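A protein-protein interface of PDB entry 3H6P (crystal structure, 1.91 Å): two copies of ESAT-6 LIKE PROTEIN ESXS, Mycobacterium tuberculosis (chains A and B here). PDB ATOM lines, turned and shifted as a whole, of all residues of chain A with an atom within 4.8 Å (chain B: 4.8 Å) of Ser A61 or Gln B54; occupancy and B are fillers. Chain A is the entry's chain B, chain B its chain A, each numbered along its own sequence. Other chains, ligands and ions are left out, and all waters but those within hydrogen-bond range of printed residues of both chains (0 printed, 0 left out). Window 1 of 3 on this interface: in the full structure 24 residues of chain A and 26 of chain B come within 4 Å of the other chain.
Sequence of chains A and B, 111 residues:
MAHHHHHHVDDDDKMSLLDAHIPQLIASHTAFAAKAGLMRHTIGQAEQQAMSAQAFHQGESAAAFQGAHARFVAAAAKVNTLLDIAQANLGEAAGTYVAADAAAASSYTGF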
ATOM      1  N   HIS A  57       9.635 -16.857  -6.630  1.00  0.00           N
ATOM      2  CA  HIS A  57      10.180 -16.157  -5.453  1.00  0.00           C
ATOM      3  C   HIS A  57      11.538 -15.488  -5.750  1.00  0.00           C
ATOM      4  O   HIS A  57      11.799 -14.379  -5.278  1.00  0.00           O
ATOM      5  CB  HIS A  57      10.323 -17.112  -4.265  1.00  0.00           C
ATOM      6  CG  HIS A  57       9.019 -17.483  -3.618  1.00  0.00           C
ATOM      7  ND1 HIS A  57       8.830 -18.679  -2.950  1.00  0.00           N
ATOM      8  CD2 HIS A  57       7.834 -16.827  -3.556  1.00  0.00           C
ATOM      9  CE1 HIS A  57       7.591 -18.735  -2.495  1.00  0.00           C
ATOM     10  NE2 HIS A  57       6.966 -17.624  -2.848  1.00  0.00           N
ATOM     11  N   GLN A  58      12.395 -16.162  -6.511  1.00  0.00           N
ATOM     12  CA  GLN A  58      13.698 -15.581  -6.890  1.00  0.00           C
ATOM     13  C   GLN A  58      13.499 -14.336  -7.765  1.00  0.00           C
ATOM     14  O   GLN A  58      14.182 -13.326  -7.588  1.00  0.00           O
ATOM     15  CB  GLN A  58      14.574 -16.604  -7.613  1.00  0.00           C
ATOM     16  CG  GLN A  58      15.110 -17.756  -6.715  1.00  0.00           C
ATOM     17  CD  GLN A  58      16.279 -17.317  -5.807  1.00  0.00           C
ATOM     18  OE1 GLN A  58      16.260 -16.224  -5.242  1.00  0.00           O
ATOM     19  NE2 GLN A  58      17.283 -18.165  -5.672  1.00  0.00           N
ATOM     20  N   GLY A  59      12.574 -14.430  -8.714  1.00  0.00           N
ATOM     21  CA  GLY A  59      12.221 -13.300  -9.586  1.00  0.00           C
ATOM     22  C   GLY A  59      11.615 -12.135  -8.829  1.00  0.00           C
ATOM     23  O   GLY A  59      11.951 -10.976  -9.100  1.00  0.00           O
ATOM     24  N   GLU A  60      10.739 -12.444  -7.875  1.00  0.00           N
ATOM     25  CA  GLU A  60      10.063 -11.442  -7.021  1.00  0.00           C
ATOM     26  C   GLU A  60      11.071 -10.688  -6.126  1.00  0.00           C
ATOM     27  O   GLU A  60      11.046  -9.452  -6.012  1.00  0.00           O
ATOM     28  CB  GLU A  60       9.022 -12.188  -6.175  1.00  0.00           C
ATOM     29  CG  GLU A  60       8.243 -11.401  -5.123  1.00  0.00           C
ATOM     30  CD  GLU A  60       7.319 -12.324  -4.314  1.00  0.00           C
ATOM     31  OE1 GLU A  60       7.825 -13.293  -3.676  1.00  0.00           O
ATOM     32  OE2 GLU A  60       6.087 -12.080  -4.318  1.00  0.00           O
ATOM     33  N   SER A  61      11.965 -11.443  -5.507  1.00  0.00           N
ATOM     34  CA  SER A  61      13.013 -10.866  -4.695  1.00  0.00           C
ATOM     35  C   SER A  61      13.931  -9.948  -5.504  1.00  0.00           C
ATOM     36  O   SER A  61      14.268  -8.863  -5.052  1.00  0.00           O
ATOM     37  CB  SER A  61      13.832 -11.966  -4.029  1.00  0.00           C
ATOM     38  OG  SER A  61      14.998 -11.400  -3.434  1.00  0.00           O
ATOM     39  N   ALA A  62      14.334 -10.387  -6.693  1.00  0.00           N
ATOM     40  CA  ALA A  62      15.193  -9.594  -7.550  1.00  0.00           C
ATOM     41  C   ALA A  62      14.478  -8.314  -8.028  1.00  0.00           C
ATOM     42  O   ALA A  62      15.053  -7.233  -7.971  1.00  0.00           O
ATOM     43  CB  ALA A  62      15.686 -10.435  -8.720  1.00  0.00           C
ATOM     44  N   ALA A  63      13.220  -8.433  -8.455  1.00  0.00           N
ATOM     45  CA  ALA A  63      12.440  -7.249  -8.897  1.00  0.00           C
ATOM     46  C   ALA A  63      12.264  -6.225  -7.781  1.00  0.00           C
ATOM     47  O   ALA A  63      12.407  -5.004  -8.032  1.00  0.00           O
ATOM     48  CB  ALA A  63      11.074  -7.677  -9.449  1.00  0.00           C
ATOM     49  N   ALA A  64      11.950  -6.711  -6.577  1.00  0.00           N
ATOM     50  CA  ALA A  64      11.749  -5.868  -5.407  1.00  0.00           C
ATOM     51  C   ALA A  64      13.050  -5.126  -5.038  1.00  0.00           C
ATOM     52  O   ALA A  64      13.026  -3.920  -4.757  1.00  0.00           O
ATOM     53  CB  ALA A  64      11.256  -6.684  -4.239  1.00  0.00           C
ATOM     54  N   PHE A  65      14.172  -5.839  -5.067  1.00  0.00           N
ATOM     55  CA  PHE A  65      15.465  -5.221  -4.765  1.00  0.00           C
ATOM     56  C   PHE A  65      15.811  -4.166  -5.811  1.00  0.00           C
ATOM     57  O   PHE A  65      16.260  -3.070  -5.487  1.00  0.00           O
ATOM     58  CB  PHE A  65      16.610  -6.255  -4.648  1.00  0.00           C
ATOM     59  CG  PHE A  65      17.939  -5.617  -4.286  1.00  0.00           C
ATOM     60  CD1 PHE A  65      18.286  -5.408  -2.964  1.00  0.00           C
ATOM     61  CD2 PHE A  65      18.798  -5.169  -5.284  1.00  0.00           C
ATOM     62  CE1 PHE A  65      19.470  -4.765  -2.646  1.00  0.00           C
ATOM     63  CE2 PHE A  65      19.988  -4.523  -4.983  1.00  0.00           C
ATOM     64  CZ  PHE A  65      20.320  -4.316  -3.662  1.00  0.00           C
ATOM     65  N   ALA B  50      24.000  -3.558   1.246  1.00  0.00           N
ATOM     66  CA  ALA B  50      22.698  -4.036   0.775  1.00  0.00           C
ATOM     67  C   ALA B  50      22.828  -4.888  -0.495  1.00  0.00           C
ATOM     68  O   ALA B  50      22.175  -5.941  -0.631  1.00  0.00           O
ATOM     69  CB  ALA B  50      21.754  -2.853   0.539  1.00  0.00           C
ATOM     70  N   MET B  51      23.676  -4.440  -1.414  1.00  0.00           N
ATOM     71  CA  MET B  51      23.940  -5.199  -2.661  1.00  0.00           C
ATOM     72  C   MET B  51      24.535  -6.567  -2.326  1.00  0.00           C
ATOM     73  O   MET B  51      24.084  -7.615  -2.830  1.00  0.00           O
ATOM     74  CB  MET B  51      24.859  -4.387  -3.588  1.00  0.00           C
ATOM     75  CG  MET B  51      24.190  -3.144  -4.193  1.00  0.00           C
ATOM     76  SD  MET B  51      25.282  -2.123  -5.287  1.00  0.00           S
ATOM     77  CE  MET B  51      25.614  -3.223  -6.534  1.00  0.00           C
ATOM     78  N   SER B  52      25.534  -6.560  -1.451  1.00  0.00           N
ATOM     79  CA  SER B  52      26.197  -7.799  -1.034  1.00  0.00           C
ATOM     80  C   SER B  52      25.233  -8.782  -0.345  1.00  0.00           C
ATOM     81  O   SER B  52      25.315  -9.993  -0.545  1.00  0.00           O
ATOM     82  CB  SER B  52      27.351  -7.486  -0.091  1.00  0.00           C
ATOM     83  OG  SER B  52      27.968  -8.690   0.302  1.00  0.00           O
ATOM     84  N   ALA B  53      24.381  -8.250   0.524  1.00  0.00           N
ATOM     85  CA  ALA B  53      23.413  -9.053   1.266  1.00  0.00           C
ATOM     86  C   ALA B  53      22.401  -9.663   0.309  1.00  0.00           C
ATOM     87  O   ALA B  53      22.004 -10.813   0.475  1.00  0.00           O
ATOM     88  CB  ALA B  53      22.713  -8.182   2.296  1.00  0.00           C
ATOM     89  N   GLN B  54      21.995  -8.917  -0.712  1.00  0.00           N
ATOM     90  CA  GLN B  54      21.016  -9.442  -1.673  1.00  0.00           C
ATOM     91  C   GLN B  54      21.651 -10.574  -2.485  1.00  0.00           C
ATOM     92  O   GLN B  54      21.030 -11.633  -2.717  1.00  0.00           O
ATOM     93  CB  GLN B  54      20.481  -8.327  -2.580  1.00  0.00           C
ATOM     94  CG  GLN B  54      19.623  -8.811  -3.758  1.00  0.00           C
ATOM     95  CD  GLN B  54      18.271  -9.347  -3.356  1.00  0.00           C
ATOM     96  OE1 GLN B  54      17.607 -10.026  -4.140  1.00  0.00           O
ATOM     97  NE2 GLN B  54      17.846  -9.044  -2.152  1.00  0.00           N
ATOM     98  N   ALA B  55      22.888 -10.371  -2.902  1.00  0.00           N
ATOM     99  CA  ALA B  55      23.584 -11.389  -3.671  1.00  0.00           C
ATOM    100  C   ALA B  55      23.733 -12.663  -2.827  1.00  0.00           C
ATOM    101  O   ALA B  55      23.487 -13.773  -3.294  1.00  0.00           O
ATOM    102  CB  ALA B  55      24.942 -10.861  -4.117  1.00  0.00           C
ATOM    103  N   PHE B  56      24.106 -12.493  -1.567  1.00  0.00           N
ATOM    104  CA  PHE B  56      24.223 -13.623  -0.636  1.00  0.00           C
ATOM    105  C   PHE B  56      22.900 -14.363  -0.466  1.00  0.00           C
ATOM    106  O   PHE B  56      22.832 -15.594  -0.552  1.00  0.00           O
ATOM    107  CB  PHE B  56      24.694 -13.110   0.727  1.00  0.00           C
ATOM    108  CG  PHE B  56      24.671 -14.156   1.799  1.00  0.00           C
ATOM    109  CD1 PHE B  56      25.532 -15.235   1.730  1.00  0.00           C
ATOM    110  CD2 PHE B  56      23.778 -14.065   2.856  1.00  0.00           C
ATOM    111  CE1 PHE B  56      25.517 -16.207   2.708  1.00  0.00           C
ATOM    112  CE2 PHE B  56      23.739 -15.047   3.825  1.00  0.00           C
ATOM    113  CZ  PHE B  56      24.614 -16.111   3.756  1.00  0.00           C
ATOM    114  N   HIS B  57      21.844 -13.614  -0.233  1.00  0.00           N
ATOM    115  CA  HIS B  57      20.541 -14.200   0.008  1.00  0.00           C
ATOM    116  C   HIS B  57      19.963 -14.917  -1.221  1.00  0.00           C
ATOM    117  O   HIS B  57      19.343 -15.982  -1.076  1.00  0.00           O
ATOM    118  CB  HIS B  57      19.602 -13.160   0.624  1.00  0.00           C
ATOM    119  CG  HIS B  57      19.895 -12.908   2.074  1.00  0.00           C
ATOM    120  ND1 HIS B  57      20.622 -11.818   2.518  1.00  0.00           N
ATOM    121  CD2 HIS B  57      19.623 -13.648   3.176  1.00  0.00           C
ATOM    122  CE1 HIS B  57      20.752 -11.885   3.833  1.00  0.00           C
ATOM    123  NE2 HIS B  57      20.152 -12.985   4.256  1.00  0.00           N
ATOM    124  N   GLN B  58      20.191 -14.379  -2.419  1.00  0.00           N
ATOM    125  CA  GLN B  58      19.792 -15.069  -3.657  1.00  0.00           C
ATOM    126  C   GLN B  58      20.521 -16.414  -3.796  1.00  0.00           C
ATOM    127  O   GLN B  58      19.907 -17.442  -4.122  1.00  0.00           O
ATOM    128  CB  GLN B  58      20.031 -14.182  -4.891  1.00  0.00           C
ATOM    129  CG  GLN B  58      18.893 -13.187  -5.162  1.00  0.00           C
ATOM    130  CD  GLN B  58      19.295 -12.029  -6.087  1.00  0.00           C
ATOM    131  OE1 GLN B  58      20.475 -11.842  -6.413  1.00  0.00           O
ATOM    132  NE2 GLN B  58      18.316 -11.235  -6.488  1.00  0.00           N
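Gln A58 touches its own counterpart, Gln B58.
Positions printed for both chains: 57 and 58.
Of the 6 pairs that touch across the chains among the printed residues, 1 has its exchanged pair printed and touching as well.
The side-chain amide oxygen (OE1) of Gln B54 sits at hydrogen-bond distance from the side-chain hydroxyl (OG) of Ser A61, at 3.0 Å.
The side-chain amide nitrogen (NE2) of Gln A58 is in hydrogen-bond range of the backbone carbonyl oxygen (O) of Gln B58 (3.1 Å).
Among the printed residues, merely in contact across the chains: Ala A62 with Gln B58, Phe A65 with Ala B50, Phe A65 with Gln B54 and Phe A65 with Met B51.
The side-chain amide nitrogen (NE2) of Gln B58 sits at hydrogen-bond distance from the side-chain amide oxygen (OE1) of Gln B54 (2.7 Å).
Of the printed residues of chain B, Ser A61 touches Gln B54 (3.0 Å).
Of chain A, only Ser A61 and Phe A65 come within 4 Å of Gln B54.
Printed residues of chain B within 4 Å of Phe A65: Ala B50, Met B51 and Gln B54.
Of the printed residues of chain B, Gln A58 touches Gln B58 (3.1 Å).
Printed residues of chain B within 4 Å of Ala A62: Gln B58.
Printed residues of chain A within 4 Å of Gln B58: Gln A58 (3.1 Å) and Ala A62 (3.5 Å).
Of the printed residues of chain A, Ala B50 touches Phe A65.
His A57 touches none of the printed residues of chain B.
The nearest printed residue of chain A that does not touch Met B51 is Ser A61 (9.9 Å).
Of the 9 printed residues of chain B, 4 touch a printed residue of chain A.
Printed residues of chain A that touch a printed residue of chain B: Gln A58, Ser A61, Ala A62 and Phe A65.
Hydrophobic or aromatic side chains of chain A that line the printed part of chain B: Ala A62 and Phe A65.
Along chain A the printed residues that touch a printed residue of chain B span positions 58 to 65.
Among the printed residues, no Asp or Glu carboxylate lies within 4 Å of a Lys or Arg side-chain nitrogen of the other chain.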
